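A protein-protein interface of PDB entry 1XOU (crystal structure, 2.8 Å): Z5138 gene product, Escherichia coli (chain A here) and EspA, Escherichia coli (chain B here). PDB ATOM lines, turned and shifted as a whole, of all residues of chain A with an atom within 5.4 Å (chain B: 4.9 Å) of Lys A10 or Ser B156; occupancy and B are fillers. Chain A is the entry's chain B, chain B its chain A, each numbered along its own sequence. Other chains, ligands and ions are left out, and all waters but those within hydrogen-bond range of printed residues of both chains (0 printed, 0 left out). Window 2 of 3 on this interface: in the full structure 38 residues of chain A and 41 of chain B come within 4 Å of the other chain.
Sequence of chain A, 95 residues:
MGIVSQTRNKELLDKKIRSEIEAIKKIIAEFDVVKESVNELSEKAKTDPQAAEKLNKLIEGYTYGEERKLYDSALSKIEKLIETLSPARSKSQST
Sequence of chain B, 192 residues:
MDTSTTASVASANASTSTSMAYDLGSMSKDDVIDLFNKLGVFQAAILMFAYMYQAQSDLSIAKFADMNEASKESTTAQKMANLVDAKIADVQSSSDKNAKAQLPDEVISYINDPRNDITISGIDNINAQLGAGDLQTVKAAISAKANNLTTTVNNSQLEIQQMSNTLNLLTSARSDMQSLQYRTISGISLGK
The side-chain amide oxygen of Gln B157 lies close to the side-chain amide oxygen of Gln A6, 2.9 Å away.
The side-chain hydroxyl (OG) of Ser B156 sits at hydrogen-bond distance from the side-chain amino group (NZ) of Lys A10, 3.2 Å away.
The side-chain carboxylate (OE2) of Glu B159 lies within salt-bridge range of the side-chain amino group (NZ) of Lys A10.
The backbone carbonyl oxygen of Val B153 sits close to the side-chain amide oxygen of Gln A6, at 2.8 Å.
OG of Ser B156 is in hydrogen-bond range of O of Thr B152, at 3.1 Å.
NE2 of Gln A6 touches CB of Ser B156 (3.4 Å).
Ile B160 touches Gln A6.
Lys A10 touches Ile B160 (CG to CG1, 3.5 Å).
Met B163 touches Lys A10 (CE to O, 3.4 Å).
Ile B160 touches Leu A13 (O to CD2, 3.7 Å).
Met B163 touches Leu A13 (CE to CB, 3.8 Å).
Asp A14 touches Met B163.
Of the printed residues of chain B, Gln A6 touches Val B153 (2.8 Å), Ser B156 (3.4 Å), Gln B157 (2.9 Å) and Ile B160 (3.8 Å).
Thr A7 touches none of the printed residues of chain B.
Lys A10 touches just these residues of chain B: Ser B156 (3.2 Å), Glu B159 (3.2 Å), Ile B160 (3.5 Å) and Met B163 (3.4 Å).
Of the printed residues of chain B, Asp A14 touches Met B163 (3.4 Å).
Of the printed residues of chain A, Val B153 touches Gln A6 (2.8 Å).
Of chain A, only Gln A6 and Lys A10 come within 4 Å of Ser B156.
Of the printed residues of chain A, Glu B159 touches Lys A10.
Printed residues of chain A within 4 Å of Ile B160: Gln A6, Lys A10 and Leu A13.
Of the 11 printed residues of chain A, 4 touch a printed residue of chain B.
Printed residues of chain A that touch a printed residue of chain B: Gln A6, Lys A10, Leu A13 and Asp A14.
Hydrophobic or aromatic side chains of chain A within 4 Å of the printed part of chain B: Leu A13.
Among the printed residues, 11 pairs touch across the chains.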
ATOM      1  N   SER A   5      -4.269  19.482 -14.117  1.00  0.00           N
ATOM      2  CA  SER A   5      -3.155  18.829 -14.817  1.00  0.00           C
ATOM      3  C   SER A   5      -2.782  17.538 -14.102  1.00  0.00           C
ATOM      4  O   SER A   5      -2.557  16.506 -14.729  1.00  0.00           O
ATOM      5  CB  SER A   5      -1.906  19.719 -14.840  1.00  0.00           C
ATOM      6  OG  SER A   5      -1.966  20.667 -15.882  1.00  0.00           O
ATOM      7  N   GLN A   6      -2.694  17.623 -12.779  1.00  0.00           N
ATOM      8  CA  GLN A   6      -2.352  16.477 -11.969  1.00  0.00           C
ATOM      9  C   GLN A   6      -3.339  15.350 -12.201  1.00  0.00           C
ATOM     10  O   GLN A   6      -2.941  14.203 -12.402  1.00  0.00           O
ATOM     11  CB  GLN A   6      -2.326  16.860 -10.491  1.00  0.00           C
ATOM     12  CG  GLN A   6      -1.009  17.457 -10.030  1.00  0.00           C
ATOM     13  CD  GLN A   6      -0.946  17.630  -8.522  1.00  0.00           C
ATOM     14  OE1 GLN A   6       0.140  17.742  -7.951  1.00  0.00           O
ATOM     15  NE2 GLN A   6      -2.112  17.659  -7.867  1.00  0.00           N
ATOM     16  N   THR A   7      -4.627  15.669 -12.180  1.00  0.00           N
ATOM     17  CA  THR A   7      -5.644  14.653 -12.406  1.00  0.00           C
ATOM     18  C   THR A   7      -5.503  14.054 -13.802  1.00  0.00           C
ATOM     19  O   THR A   7      -5.610  12.841 -13.983  1.00  0.00           O
ATOM     20  CB  THR A   7      -7.044  15.231 -12.268  1.00  0.00           C
ATOM     21  OG1 THR A   7      -7.166  15.870 -10.992  1.00  0.00           O
ATOM     22  CG2 THR A   7      -8.080  14.122 -12.375  1.00  0.00           C
ATOM     23  N   ARG A   8      -5.270  14.901 -14.795  1.00  0.00           N
ATOM     24  CA  ARG A   8      -5.111  14.403 -16.150  1.00  0.00           C
ATOM     25  C   ARG A   8      -3.913  13.458 -16.220  1.00  0.00           C
ATOM     26  O   ARG A   8      -3.970  12.424 -16.873  1.00  0.00           O
ATOM     27  CB  ARG A   8      -4.935  15.562 -17.140  1.00  0.00           C
ATOM     28  CG  ARG A   8      -4.755  15.087 -18.567  1.00  0.00           C
ATOM     29  CD  ARG A   8      -5.337  16.042 -19.589  1.00  0.00           C
ATOM     30  NE  ARG A   8      -5.408  15.407 -20.909  1.00  0.00           N
ATOM     31  CZ  ARG A   8      -5.893  15.985 -22.009  1.00  0.00           C
ATOM     32  NH1 ARG A   8      -5.909  15.309 -23.156  1.00  0.00           N
ATOM     33  NH2 ARG A   8      -6.360  17.232 -21.967  1.00  0.00           N
ATOM     34  N   ASN A   9      -2.828  13.802 -15.539  1.00  0.00           N
ATOM     35  CA  ASN A   9      -1.649  12.949 -15.550  1.00  0.00           C
ATOM     36  C   ASN A   9      -1.872  11.624 -14.834  1.00  0.00           C
ATOM     37  O   ASN A   9      -1.380  10.595 -15.276  1.00  0.00           O
ATOM     38  CB  ASN A   9      -0.459  13.671 -14.927  1.00  0.00           C
ATOM     39  CG  ASN A   9       0.250  14.575 -15.912  1.00  0.00           C
ATOM     40  OD1 ASN A   9       0.968  15.493 -15.513  1.00  0.00           O
ATOM     41  ND2 ASN A   9       0.069  14.315 -17.206  1.00  0.00           N
ATOM     42  N   LYS A  10      -2.606  11.638 -13.729  1.00  0.00           N
ATOM     43  CA  LYS A  10      -2.857  10.405 -13.007  1.00  0.00           C
ATOM     44  C   LYS A  10      -3.726   9.473 -13.835  1.00  0.00           C
ATOM     45  O   LYS A  10      -3.545   8.260 -13.800  1.00  0.00           O
ATOM     46  CB  LYS A  10      -3.496  10.713 -11.652  1.00  0.00           C
ATOM     47  CG  LYS A  10      -2.483  11.301 -10.671  1.00  0.00           C
ATOM     48  CD  LYS A  10      -3.087  12.215  -9.599  1.00  0.00           C
ATOM     49  CE  LYS A  10      -3.783  11.450  -8.484  1.00  0.00           C
ATOM     50  NZ  LYS A  10      -4.092  12.361  -7.337  1.00  0.00           N
ATOM     51  N   GLU A  11      -4.652  10.044 -14.601  1.00  0.00           N
ATOM     52  CA  GLU A  11      -5.537   9.255 -15.457  1.00  0.00           C
ATOM     53  C   GLU A  11      -4.747   8.615 -16.596  1.00  0.00           C
ATOM     54  O   GLU A  11      -4.975   7.463 -16.951  1.00  0.00           O
ATOM     55  CB  GLU A  11      -6.635  10.134 -16.048  1.00  0.00           C
ATOM     56  CG  GLU A  11      -7.613  10.698 -15.042  1.00  0.00           C
ATOM     57  CD  GLU A  11      -8.715  11.496 -15.718  1.00  0.00           C
ATOM     58  OE1 GLU A  11      -9.400  10.921 -16.595  1.00  0.00           O
ATOM     59  OE2 GLU A  11      -8.897  12.693 -15.382  1.00  0.00           O
ATOM     60  N   LEU A  12      -3.834   9.383 -17.177  1.00  0.00           N
ATOM     61  CA  LEU A  12      -2.981   8.914 -18.261  1.00  0.00           C
ATOM     62  C   LEU A  12      -2.204   7.691 -17.782  1.00  0.00           C
ATOM     63  O   LEU A  12      -2.297   6.609 -18.366  1.00  0.00           O
ATOM     64  CB  LEU A  12      -1.998  10.023 -18.638  1.00  0.00           C
ATOM     65  CG  LEU A  12      -2.160  10.801 -19.947  1.00  0.00           C
ATOM     66  CD1 LEU A  12      -1.423  10.054 -21.056  1.00  0.00           C
ATOM     67  CD2 LEU A  12      -3.638  11.006 -20.275  1.00  0.00           C
ATOM     68  N   LEU A  13      -1.430   7.891 -16.715  1.00  0.00           N
ATOM     69  CA  LEU A  13      -0.625   6.843 -16.102  1.00  0.00           C
ATOM     70  C   LEU A  13      -1.478   5.616 -15.824  1.00  0.00           C
ATOM     71  O   LEU A  13      -1.163   4.514 -16.267  1.00  0.00           O
ATOM     72  CB  LEU A  13      -0.005   7.354 -14.795  1.00  0.00           C
ATOM     73  CG  LEU A  13       1.439   7.891 -14.809  1.00  0.00           C
ATOM     74  CD1 LEU A  13       1.951   8.065 -16.222  1.00  0.00           C
ATOM     75  CD2 LEU A  13       1.496   9.207 -14.058  1.00  0.00           C
ATOM     76  N   ASP A  14      -2.565   5.808 -15.092  1.00  0.00           N
ATOM     77  CA  ASP A  14      -3.447   4.700 -14.772  1.00  0.00           C
ATOM     78  C   ASP A  14      -3.851   3.926 -16.026  1.00  0.00           C
ATOM     79  O   ASP A  14      -3.751   2.707 -16.061  1.00  0.00           O
ATOM     80  CB  ASP A  14      -4.675   5.225 -14.038  1.00  0.00           C
ATOM     81  CG  ASP A  14      -5.693   4.153 -13.778  1.00  0.00           C
ATOM     82  OD1 ASP A  14      -6.569   3.960 -14.651  1.00  0.00           O
ATOM     83  OD2 ASP A  14      -5.611   3.501 -12.710  1.00  0.00           O
ATOM     84  N   LYS A  15      -4.295   4.632 -17.060  1.00  0.00           N
ATOM     85  CA  LYS A  15      -4.693   3.973 -18.297  1.00  0.00           C
ATOM     86  C   LYS A  15      -3.512   3.239 -18.916  1.00  0.00           C
ATOM     87  O   LYS A  15      -3.653   2.119 -19.396  1.00  0.00           O
ATOM     88  CB  LYS A  15      -5.237   4.988 -19.315  1.00  0.00           C
ATOM     89  CG  LYS A  15      -6.608   5.577 -18.996  1.00  0.00           C
ATOM     90  CD  LYS A  15      -7.031   6.538 -20.108  1.00  0.00           C
ATOM     91  CE  LYS A  15      -8.200   7.443 -19.701  1.00  0.00           C
ATOM     92  NZ  LYS A  15      -8.391   8.579 -20.663  1.00  0.00           N
ATOM     93  N   THR B 151      -0.210  20.203   0.858  1.00  0.00           N
ATOM     94  CA  THR B 151      -0.006  18.791   1.128  1.00  0.00           C
ATOM     95  C   THR B 151      -0.607  18.010  -0.039  1.00  0.00           C
ATOM     96  O   THR B 151       0.074  17.232  -0.712  1.00  0.00           O
ATOM     97  CB  THR B 151      -0.714  18.387   2.446  1.00  0.00           C
ATOM     98  OG1 THR B 151       0.025  18.896   3.560  1.00  0.00           O
ATOM     99  CG2 THR B 151      -0.826  16.880   2.558  1.00  0.00           C
ATOM    100  N   THR B 152      -1.893  18.249  -0.267  1.00  0.00           N
ATOM    101  CA  THR B 152      -2.642  17.607  -1.331  1.00  0.00           C
ATOM    102  C   THR B 152      -1.926  17.643  -2.669  1.00  0.00           C
ATOM    103  O   THR B 152      -1.862  16.640  -3.371  1.00  0.00           O
ATOM    104  CB  THR B 152      -4.004  18.282  -1.487  1.00  0.00           C
ATOM    105  OG1 THR B 152      -4.750  18.095  -0.279  1.00  0.00           O
ATOM    106  CG2 THR B 152      -4.772  17.703  -2.676  1.00  0.00           C
ATOM    107  N   VAL B 153      -1.401  18.808  -3.021  1.00  0.00           N
ATOM    108  CA  VAL B 153      -0.696  18.971  -4.285  1.00  0.00           C
ATOM    109  C   VAL B 153       0.608  18.187  -4.301  1.00  0.00           C
ATOM    110  O   VAL B 153       1.031  17.692  -5.345  1.00  0.00           O
ATOM    111  CB  VAL B 153      -0.408  20.477  -4.569  1.00  0.00           C
ATOM    112  CG1 VAL B 153       0.631  20.635  -5.685  1.00  0.00           C
ATOM    113  CG2 VAL B 153      -1.700  21.169  -4.960  1.00  0.00           C
ATOM    114  N   ASN B 154       1.240  18.065  -3.141  1.00  0.00           N
ATOM    115  CA  ASN B 154       2.495  17.344  -3.052  1.00  0.00           C
ATOM    116  C   ASN B 154       2.288  15.840  -3.056  1.00  0.00           C
ATOM    117  O   ASN B 154       3.023  15.112  -3.727  1.00  0.00           O
ATOM    118  CB  ASN B 154       3.264  17.784  -1.805  1.00  0.00           C
ATOM    119  CG  ASN B 154       3.798  19.207  -1.923  1.00  0.00           C
ATOM    120  OD1 ASN B 154       4.074  19.867  -0.918  1.00  0.00           O
ATOM    121  ND2 ASN B 154       3.953  19.682  -3.157  1.00  0.00           N
ATOM    122  N   ASN B 155       1.286  15.366  -2.326  1.00  0.00           N
ATOM    123  CA  ASN B 155       1.031  13.934  -2.296  1.00  0.00           C
ATOM    124  C   ASN B 155       0.725  13.408  -3.697  1.00  0.00           C
ATOM    125  O   ASN B 155       1.207  12.346  -4.097  1.00  0.00           O
ATOM    126  CB  ASN B 155      -0.126  13.611  -1.352  1.00  0.00           C
ATOM    127  CG  ASN B 155       0.169  14.010   0.084  1.00  0.00           C
ATOM    128  OD1 ASN B 155       1.325  13.972   0.536  1.00  0.00           O
ATOM    129  ND2 ASN B 155      -0.877  14.386   0.820  1.00  0.00           N
ATOM    130  N   SER B 156      -0.074  14.161  -4.443  1.00  0.00           N
ATOM    131  CA  SER B 156      -0.426  13.773  -5.795  1.00  0.00           C
ATOM    132  C   SER B 156       0.804  13.772  -6.680  1.00  0.00           C
ATOM    133  O   SER B 156       0.963  12.900  -7.528  1.00  0.00           O
ATOM    134  CB  SER B 156      -1.466  14.729  -6.358  1.00  0.00           C
ATOM    135  OG  SER B 156      -2.645  14.647  -5.588  1.00  0.00           O
ATOM    136  N   GLN B 157       1.679  14.747  -6.489  1.00  0.00           N
ATOM    137  CA  GLN B 157       2.873  14.802  -7.305  1.00  0.00           C
ATOM    138  C   GLN B 157       3.700  13.549  -7.037  1.00  0.00           C
ATOM    139  O   GLN B 157       4.343  13.010  -7.937  1.00  0.00           O
ATOM    140  CB  GLN B 157       3.675  16.062  -6.989  1.00  0.00           C
ATOM    141  CG  GLN B 157       4.453  16.565  -8.185  1.00  0.00           C
ATOM    142  CD  GLN B 157       3.639  16.464  -9.476  1.00  0.00           C
ATOM    143  OE1 GLN B 157       2.473  16.873  -9.524  1.00  0.00           O
ATOM    144  NE2 GLN B 157       4.255  15.920 -10.529  1.00  0.00           N
ATOM    145  N   LEU B 158       3.664  13.082  -5.792  1.00  0.00           N
ATOM    146  CA  LEU B 158       4.382  11.876  -5.392  1.00  0.00           C
ATOM    147  C   LEU B 158       3.754  10.628  -6.018  1.00  0.00           C
ATOM    148  O   LEU B 158       4.463   9.736  -6.475  1.00  0.00           O
ATOM    149  CB  LEU B 158       4.378  11.755  -3.871  1.00  0.00           C
ATOM    150  CG  LEU B 158       5.742  11.882  -3.186  1.00  0.00           C
ATOM    151  CD1 LEU B 158       6.578  12.998  -3.822  1.00  0.00           C
ATOM    152  CD2 LEU B 158       5.510  12.140  -1.707  1.00  0.00           C
ATOM    153  N   GLU B 159       2.424  10.570  -6.033  1.00  0.00           N
ATOM    154  CA  GLU B 159       1.706   9.449  -6.629  1.00  0.00           C
ATOM    155  C   GLU B 159       2.049   9.370  -8.111  1.00  0.00           C
ATOM    156  O   GLU B 159       2.251   8.289  -8.662  1.00  0.00           O
ATOM    157  CB  GLU B 159       0.204   9.641  -6.484  1.00  0.00           C
ATOM    158  CG  GLU B 159      -0.243   9.904  -5.066  1.00  0.00           C
ATOM    159  CD  GLU B 159      -1.737  10.191  -4.974  1.00  0.00           C
ATOM    160  OE1 GLU B 159      -2.201  10.607  -3.883  1.00  0.00           O
ATOM    161  OE2 GLU B 159      -2.443   9.995  -5.994  1.00  0.00           O
ATOM    162  N   ILE B 160       2.108  10.530  -8.754  1.00  0.00           N
ATOM    163  CA  ILE B 160       2.427  10.597 -10.170  1.00  0.00           C
ATOM    164  C   ILE B 160       3.841  10.076 -10.410  1.00  0.00           C
ATOM    165  O   ILE B 160       4.106   9.442 -11.435  1.00  0.00           O
ATOM    166  CB  ILE B 160       2.284  12.052 -10.693  1.00  0.00           C
ATOM    167  CG1 ILE B 160       0.822  12.500 -10.565  1.00  0.00           C
ATOM    168  CG2 ILE B 160       2.735  12.142 -12.143  1.00  0.00           C
ATOM    169  CD1 ILE B 160       0.554  13.901 -11.062  1.00  0.00           C
ATOM    170  N   MET B 163       3.526   6.131  -9.758  1.00  0.00           N
ATOM    171  CA  MET B 163       2.791   5.582 -10.899  1.00  0.00           C
ATOM    172  C   MET B 163       3.656   5.553 -12.151  1.00  0.00           C
ATOM    173  O   MET B 163       3.585   4.627 -12.959  1.00  0.00           O
ATOM    174  CB  MET B 163       1.543   6.416 -11.184  1.00  0.00           C
ATOM    175  CG  MET B 163       0.495   6.324 -10.103  1.00  0.00           C
ATOM    176  SD  MET B 163      -1.115   7.340 -10.506  1.00  0.00           S
ATOM    177  CE  MET B 163      -1.953   6.086 -11.734  1.00  0.00           C
